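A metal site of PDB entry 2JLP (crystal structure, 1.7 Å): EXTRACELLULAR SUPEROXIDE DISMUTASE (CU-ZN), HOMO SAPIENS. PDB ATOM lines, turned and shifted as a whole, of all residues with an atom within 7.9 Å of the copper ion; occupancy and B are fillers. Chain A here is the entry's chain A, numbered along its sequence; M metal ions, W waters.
A ring nitrogen (NE2) of His 98 binds the copper ion (2.0 Å). NE2 of His 163 is bound to the copper ion, at 2.1 Å. A ring nitrogen (ND1) of His 96 is bound to the copper ion.
His 113 touches the copper ion. Of the 26 residues printed, 4 come within 4 Å of the copper ion. The nearest printed residue that does not touch the copper ion is Val 161 (4.1 Å).
ND1 of His 98 sits close to NH2 of Arg 186. ND1 of His 98 lies within hydrogen-bond range of O of Gly 111 (2.8 Å). The backbone NH of His 163 lies within hydrogen-bond range of the backbone carbonyl oxygen of Ala 94. A ring nitrogen (ND1) of His 163 sits at hydrogen-bond distance from the backbone carbonyl oxygen (O) of Gly 184 (2.9 Å). A ring nitrogen (ND1) of His 163 lies close to the backbone carbonyl oxygen (O) of Arg 185 (3.5 Å). ND1 of His 96 lies close to NE2 of His 113, 3.1 Å away. The backbone NH (N) of Val 161 lies within hydrogen-bond range of the backbone carbonyl oxygen (O) of His 96, at 2.8 Å. NE2 of His 96 lies within hydrogen-bond range of OD2 of Asp 167 (2.7 Å).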
ATOM      1  N   ALA A  94      -4.928 -22.972  14.099  1.00  0.00           N
ATOM      2  CA  ALA A  94      -3.610 -22.413  13.759  1.00  0.00           C
ATOM      3  C   ALA A  94      -3.661 -20.861  13.699  1.00  0.00           C
ATOM      4  O   ALA A  94      -4.601 -20.294  13.149  1.00  0.00           O
ATOM      5  CB  ALA A  94      -3.133 -22.952  12.431  1.00  0.00           C
ATOM      6  N   ILE A  95      -2.603 -20.188  14.158  1.00  0.00           N
ATOM      7  CA  ILE A  95      -2.425 -18.766  13.971  1.00  0.00           C
ATOM      8  C   ILE A  95      -0.999 -18.512  13.475  1.00  0.00           C
ATOM      9  O   ILE A  95      -0.041 -19.066  14.046  1.00  0.00           O
ATOM     10  CB  ILE A  95      -2.674 -17.975  15.249  1.00  0.00           C
ATOM     11  CG1 ILE A  95      -4.103 -18.310  15.789  1.00  0.00           C
ATOM     12  CG2 ILE A  95      -2.491 -16.503  14.958  1.00  0.00           C
ATOM     13  CD1 ILE A  95      -4.483 -17.661  17.143  1.00  0.00           C
ATOM     14  N   HIS A  96      -0.879 -17.695  12.428  1.00  0.00           N
ATOM     15  CA  HIS A  96       0.440 -17.400  11.890  1.00  0.00           C
ATOM     16  C   HIS A  96       0.567 -15.942  11.461  1.00  0.00           C
ATOM     17  O   HIS A  96      -0.443 -15.307  11.181  1.00  0.00           O
ATOM     18  CB  HIS A  96       0.689 -18.203  10.620  1.00  0.00           C
ATOM     19  CG  HIS A  96       0.281 -19.649  10.648  1.00  0.00           C
ATOM     20  ND1 HIS A  96      -0.672 -20.135   9.794  1.00  0.00           N
ATOM     21  CD2 HIS A  96       0.805 -20.718  11.301  1.00  0.00           C
ATOM     22  CE1 HIS A  96      -0.756 -21.446   9.946  1.00  0.00           C
ATOM     23  NE2 HIS A  96       0.106 -21.827  10.868  1.00  0.00           N
ATOM     24  N   VAL A  97       1.793 -15.562  11.128  1.00  0.00           N
ATOM     25  CA  VAL A  97       2.046 -14.276  10.477  1.00  0.00           C
ATOM     26  C   VAL A  97       2.195 -14.533   8.966  1.00  0.00           C
ATOM     27  O   VAL A  97       2.993 -15.388   8.558  1.00  0.00           O
ATOM     28  CB  VAL A  97       3.324 -13.570  11.004  1.00  0.00           C
ATOM     29  CG1 VAL A  97       3.567 -12.287  10.270  1.00  0.00           C
ATOM     30  CG2 VAL A  97       3.289 -13.342  12.538  1.00  0.00           C
ATOM     31  N   HIS A  98       1.460 -13.766   8.171  1.00  0.00           N
ATOM     32  CA  HIS A  98       1.482 -13.758   6.725  1.00  0.00           C
ATOM     33  C   HIS A  98       2.168 -12.482   6.237  1.00  0.00           C
ATOM     34  O   HIS A  98       2.273 -11.439   6.980  1.00  0.00           O
ATOM     35  CB  HIS A  98       0.097 -13.922   6.146  1.00  0.00           C
ATOM     36  CG  HIS A  98      -0.449 -15.279   6.358  1.00  0.00           C
ATOM     37  ND1 HIS A  98      -0.848 -16.100   5.317  1.00  0.00           N
ATOM     38  CD2 HIS A  98      -0.605 -16.002   7.497  1.00  0.00           C
ATOM     39  CE1 HIS A  98      -1.260 -17.248   5.812  1.00  0.00           C
ATOM     40  NE2 HIS A  98      -1.144 -17.217   7.113  1.00  0.00           N
ATOM     41  N   THR A 110      -3.305 -11.318   2.144  1.00  0.00           N
ATOM     42  CA  THR A 110      -2.149 -11.228   3.044  1.00  0.00           C
ATOM     43  C   THR A 110      -0.978 -12.067   2.566  1.00  0.00           C
ATOM     44  O   THR A 110       0.082 -11.979   3.149  1.00  0.00           O
ATOM     45  CB  THR A 110      -2.502 -11.580   4.486  1.00  0.00           C
ATOM     46  OG1 THR A 110      -2.876 -12.960   4.564  1.00  0.00           O
ATOM     47  CG2 THR A 110      -3.661 -10.679   5.008  1.00  0.00           C
ATOM     48  N   GLY A 111      -1.157 -12.870   1.516  1.00  0.00           N
ATOM     49  CA  GLY A 111      -0.043 -13.593   0.981  1.00  0.00           C
ATOM     50  C   GLY A 111       0.296 -14.857   1.782  1.00  0.00           C
ATOM     51  O   GLY A 111      -0.489 -15.341   2.599  1.00  0.00           O
ATOM     52  N   PRO A 112       1.484 -15.420   1.531  1.00  0.00           N
ATOM     53  CA  PRO A 112       1.866 -16.642   2.218  1.00  0.00           C
ATOM     54  C   PRO A 112       2.475 -16.363   3.573  1.00  0.00           C
ATOM     55  O   PRO A 112       2.536 -15.165   3.933  1.00  0.00           O
ATOM     56  CB  PRO A 112       2.952 -17.194   1.311  1.00  0.00           C
ATOM     57  CG  PRO A 112       3.574 -16.006   0.751  1.00  0.00           C
ATOM     58  CD  PRO A 112       2.499 -14.992   0.582  1.00  0.00           C
ATOM     59  N   HIS A 113       2.934 -17.409   4.285  1.00  0.00           N
ATOM     60  CA  HIS A 113       3.537 -17.197   5.616  1.00  0.00           C
ATOM     61  C   HIS A 113       4.752 -16.293   5.386  1.00  0.00           C
ATOM     62  O   HIS A 113       5.477 -16.458   4.389  1.00  0.00           O
ATOM     63  CB  HIS A 113       3.952 -18.520   6.252  1.00  0.00           C
ATOM     64  CG  HIS A 113       2.797 -19.351   6.685  1.00  0.00           C
ATOM     65  ND1 HIS A 113       2.908 -20.403   7.559  1.00  0.00           N
ATOM     66  CD2 HIS A 113       1.469 -19.243   6.367  1.00  0.00           C
ATOM     67  CE1 HIS A 113       1.709 -20.931   7.758  1.00  0.00           C
ATOM     68  NE2 HIS A 113       0.813 -20.223   7.075  1.00  0.00           N
ATOM     69  N   TYR A 114       4.985 -15.338   6.293  1.00  0.00           N
ATOM     70  CA  TYR A 114       6.113 -14.452   6.149  1.00  0.00           C
ATOM     71  C   TYR A 114       7.388 -15.295   6.287  1.00  0.00           C
ATOM     72  O   TYR A 114       7.568 -16.016   7.255  1.00  0.00           O
ATOM     73  CB  TYR A 114       6.035 -13.335   7.207  1.00  0.00           C
ATOM     74  CG  TYR A 114       7.237 -12.434   7.230  1.00  0.00           C
ATOM     75  CD1 TYR A 114       7.727 -11.851   6.066  1.00  0.00           C
ATOM     76  CD2 TYR A 114       7.884 -12.105   8.443  1.00  0.00           C
ATOM     77  CE1 TYR A 114       8.780 -10.983   6.100  1.00  0.00           C
ATOM     78  CE2 TYR A 114       8.960 -11.232   8.484  1.00  0.00           C
ATOM     79  CZ  TYR A 114       9.413 -10.672   7.312  1.00  0.00           C
ATOM     80  OH  TYR A 114      10.536  -9.836   7.272  1.00  0.00           O
ATOM     81  N   HIS A 121       7.873 -24.330   6.199  1.00  0.00           N
ATOM     82  CA  HIS A 121       7.056 -24.457   7.367  1.00  0.00           C
ATOM     83  C   HIS A 121       7.404 -25.726   8.123  1.00  0.00           C
ATOM     84  O   HIS A 121       7.610 -26.805   7.487  1.00  0.00           O
ATOM     85  CB  HIS A 121       5.576 -24.524   6.934  1.00  0.00           C
ATOM     86  CG  HIS A 121       4.596 -24.464   8.072  1.00  0.00           C
ATOM     87  ND1 HIS A 121       4.180 -23.281   8.669  1.00  0.00           N
ATOM     88  CD2 HIS A 121       3.951 -25.465   8.710  1.00  0.00           C
ATOM     89  CE1 HIS A 121       3.350 -23.588   9.651  1.00  0.00           C
ATOM     90  NE2 HIS A 121       3.150 -24.901   9.669  1.00  0.00           N
ATOM     91  N   GLY A 126       6.885 -16.407  12.203  1.00  0.00           N
ATOM     92  CA  GLY A 126       5.502 -16.199  12.682  1.00  0.00           C
ATOM     93  C   GLY A 126       4.668 -17.457  12.754  1.00  0.00           C
ATOM     94  O   GLY A 126       3.418 -17.388  12.882  1.00  0.00           O
ATOM     95  N   ASP A 127       5.320 -18.628  12.699  1.00  0.00           N
ATOM     96  CA  ASP A 127       4.630 -19.890  12.899  1.00  0.00           C
ATOM     97  C   ASP A 127       4.310 -20.112  14.385  1.00  0.00           C
ATOM     98  O   ASP A 127       5.060 -20.807  15.058  1.00  0.00           O
ATOM     99  CB  ASP A 127       5.449 -21.046  12.354  1.00  0.00           C
ATOM    100  CG  ASP A 127       5.457 -21.082  10.880  1.00  0.00           C
ATOM    101  OD1 ASP A 127       4.480 -20.565  10.253  1.00  0.00           O
ATOM    102  OD2 ASP A 127       6.428 -21.659  10.293  1.00  0.00           O
ATOM    103  N   ALA A 159       0.627  -9.304   8.689  1.00  0.00           N
ATOM    104  CA  ALA A 159      -0.735  -9.785   9.047  1.00  0.00           C
ATOM    105  C   ALA A 159      -0.660 -10.942  10.018  1.00  0.00           C
ATOM    106  O   ALA A 159       0.206 -11.803   9.898  1.00  0.00           O
ATOM    107  CB  ALA A 159      -1.553 -10.218   7.760  1.00  0.00           C
ATOM    108  N   VAL A 160      -1.575 -10.989  10.983  1.00  0.00           N
ATOM    109  CA  VAL A 160      -1.782 -12.195  11.769  1.00  0.00           C
ATOM    110  C   VAL A 160      -3.031 -12.798  11.156  1.00  0.00           C
ATOM    111  O   VAL A 160      -4.021 -12.090  10.909  1.00  0.00           O
ATOM    112  CB  VAL A 160      -1.958 -11.947  13.304  1.00  0.00           C
ATOM    113  CG1 VAL A 160      -2.510 -13.182  13.974  1.00  0.00           C
ATOM    114  CG2 VAL A 160      -0.588 -11.485  13.913  1.00  0.00           C
ATOM    115  N   VAL A 161      -2.969 -14.086  10.856  1.00  0.00           N
ATOM    116  CA  VAL A 161      -4.082 -14.822  10.299  1.00  0.00           C
ATOM    117  C   VAL A 161      -4.483 -16.015  11.179  1.00  0.00           C
ATOM    118  O   VAL A 161      -3.623 -16.810  11.598  1.00  0.00           O
ATOM    119  CB  VAL A 161      -3.800 -15.308   8.855  1.00  0.00           C
ATOM    120  CG1 VAL A 161      -5.048 -16.109   8.300  1.00  0.00           C
ATOM    121  CG2 VAL A 161      -3.509 -14.081   7.922  1.00  0.00           C
ATOM    122  N   VAL A 162      -5.786 -16.111  11.467  1.00  0.00           N
ATOM    123  CA  VAL A 162      -6.358 -17.196  12.249  1.00  0.00           C
ATOM    124  C   VAL A 162      -7.077 -18.158  11.280  1.00  0.00           C
ATOM    125  O   VAL A 162      -7.856 -17.721  10.407  1.00  0.00           O
ATOM    126  CB  VAL A 162      -7.443 -16.667  13.224  1.00  0.00           C
ATOM    127  CG1 VAL A 162      -8.067 -17.803  14.005  1.00  0.00           C
ATOM    128  CG2 VAL A 162      -6.837 -15.640  14.200  1.00  0.00           C
ATOM    129  N   HIS A 163      -6.737 -19.454  11.362  1.00  0.00           N
ATOM    130  CA  HIS A 163      -7.251 -20.500  10.438  1.00  0.00           C
ATOM    131  C   HIS A 163      -8.341 -21.340  11.013  1.00  0.00           C
ATOM    132  O   HIS A 163      -8.567 -21.380  12.199  1.00  0.00           O
ATOM    133  CB  HIS A 163      -6.120 -21.391  10.007  1.00  0.00           C
ATOM    134  CG  HIS A 163      -5.103 -20.722   9.156  1.00  0.00           C
ATOM    135  ND1 HIS A 163      -5.179 -20.728   7.790  1.00  0.00           N
ATOM    136  CD2 HIS A 163      -3.972 -20.027   9.469  1.00  0.00           C
ATOM    137  CE1 HIS A 163      -4.113 -20.135   7.287  1.00  0.00           C
ATOM    138  NE2 HIS A 163      -3.414 -19.633   8.289  1.00  0.00           N
ATOM    139  N   ASP A 167      -2.714 -26.962  12.475  1.00  0.00           N
ATOM    140  CA  ASP A 167      -1.438 -26.914  11.805  1.00  0.00           C
ATOM    141  C   ASP A 167      -0.776 -28.284  12.025  1.00  0.00           C
ATOM    142  O   ASP A 167      -0.573 -28.741  13.165  1.00  0.00           O
ATOM    143  CB  ASP A 167      -0.599 -25.831  12.496  1.00  0.00           C
ATOM    144  CG  ASP A 167       0.670 -25.450  11.726  1.00  0.00           C
ATOM    145  OD1 ASP A 167       1.333 -26.306  11.146  1.00  0.00           O
ATOM    146  OD2 ASP A 167       0.987 -24.259  11.720  1.00  0.00           O
ATOM    147  N   GLU A 179       4.341 -25.749   3.539  1.00  0.00           N
ATOM    148  CA  GLU A 179       4.087 -24.343   3.214  1.00  0.00           C
ATOM    149  C   GLU A 179       3.286 -23.681   4.321  1.00  0.00           C
ATOM    150  O   GLU A 179       3.614 -22.581   4.730  1.00  0.00           O
ATOM    151  CB  GLU A 179       3.367 -24.232   1.856  1.00  0.00           C
ATOM    152  CG  GLU A 179       4.159 -24.880   0.745  1.00  0.00           C
ATOM    153  CD  GLU A 179       5.439 -24.129   0.372  1.00  0.00           C
ATOM    154  OE1 GLU A 179       5.559 -22.945   0.685  1.00  0.00           O
ATOM    155  OE2 GLU A 179       6.327 -24.750  -0.220  1.00  0.00           O
ATOM    156  N   ASN A 180       2.206 -24.344   4.768  1.00  0.00           N
ATOM    157  CA  ASN A 180       1.261 -23.745   5.711  1.00  0.00           C
ATOM    158  C   ASN A 180       0.677 -24.713   6.710  1.00  0.00           C
ATOM    159  O   ASN A 180      -0.210 -24.349   7.451  1.00  0.00           O
ATOM    160  CB  ASN A 180       0.122 -23.075   4.952  1.00  0.00           C
ATOM    161  CG  ASN A 180      -0.611 -24.001   4.026  1.00  0.00           C
ATOM    162  OD1 ASN A 180      -0.924 -25.168   4.340  1.00  0.00           O
ATOM    163  ND2 ASN A 180      -0.948 -23.476   2.844  1.00  0.00           N
ATOM    164  N   ALA A 183      -3.356 -25.877   7.459  1.00  0.00           N
ATOM    165  CA  ALA A 183      -4.163 -25.213   8.452  1.00  0.00           C
ATOM    166  C   ALA A 183      -5.520 -24.789   7.920  1.00  0.00           C
ATOM    167  O   ALA A 183      -6.395 -24.391   8.688  1.00  0.00           O
ATOM    168  CB  ALA A 183      -3.413 -24.043   9.056  1.00  0.00           C
ATOM    169  N   GLY A 184      -5.722 -24.883   6.611  1.00  0.00           N
ATOM    170  CA  GLY A 184      -7.027 -24.613   6.012  1.00  0.00           C
ATOM    171  C   GLY A 184      -7.383 -23.134   5.861  1.00  0.00           C
ATOM    172  O   GLY A 184      -6.532 -22.254   5.739  1.00  0.00           O
ATOM    173  N   ARG A 185      -8.692 -22.899   5.840  1.00  0.00           N
ATOM    174  CA  ARG A 185      -9.219 -21.639   5.389  1.00  0.00           C
ATOM    175  C   ARG A 185      -8.875 -20.516   6.376  1.00  0.00           C
ATOM    176  O   ARG A 185      -8.661 -20.761   7.541  1.00  0.00           O
ATOM    177  CB  ARG A 185     -10.721 -21.776   5.132  1.00  0.00           C
ATOM    178  CG  ARG A 185     -11.037 -22.736   3.969  1.00  0.00           C
ATOM    179  CD  ARG A 185     -12.519 -23.020   3.810  1.00  0.00           C
ATOM    180  NE  ARG A 185     -13.197 -21.916   3.144  1.00  0.00           N
ATOM    181  CZ  ARG A 185     -14.504 -21.790   3.035  1.00  0.00           C
ATOM    182  NH1 ARG A 185     -15.330 -22.655   3.604  1.00  0.00           N
ATOM    183  NH2 ARG A 185     -15.009 -20.736   2.386  1.00  0.00           N
ATOM    184  N   ARG A 186      -8.739 -19.291   5.848  1.00  0.00           N
ATOM    185  CA  ARG A 186      -8.333 -18.097   6.609  1.00  0.00           C
ATOM    186  C   ARG A 186      -9.645 -17.427   7.097  1.00  0.00           C
ATOM    187  O   ARG A 186     -10.466 -17.036   6.295  1.00  0.00           O
ATOM    188  CB  ARG A 186      -7.531 -17.139   5.742  1.00  0.00           C
ATOM    189  CG  ARG A 186      -6.276 -17.728   5.221  1.00  0.00           C
ATOM    190  CD  ARG A 186      -5.583 -16.832   4.204  1.00  0.00           C
ATOM    191  NE  ARG A 186      -4.410 -17.506   3.617  1.00  0.00           N
ATOM    192  CZ  ARG A 186      -3.375 -16.861   3.038  1.00  0.00           C
ATOM    193  NH1 ARG A 186      -3.392 -15.538   2.888  1.00  0.00           N
ATOM    194  NH2 ARG A 186      -2.339 -17.565   2.555  1.00  0.00           N
ATOM    195  N   ALA A 188      -9.901 -15.107   9.870  1.00  0.00           N
ATOM    196  CA  ALA A 188      -9.885 -13.742  10.444  1.00  0.00           C
ATOM    197  C   ALA A 188      -8.469 -13.266  10.494  1.00  0.00           C
ATOM    198  O   ALA A 188      -7.525 -14.086  10.451  1.00  0.00           O
ATOM    199  CB  ALA A 188     -10.591 -13.754  11.867  1.00  0.00           C
HETATM  200 CU    CU M   1      -1.568 -18.688   8.446  1.00  0.00          CU
HETATM  201 ZN    ZN M   2       4.584 -21.208   8.306  1.00  0.00          ZN
HETATM  202  O   HOH W   1      -1.567 -20.470   5.482  1.00  0.00           O
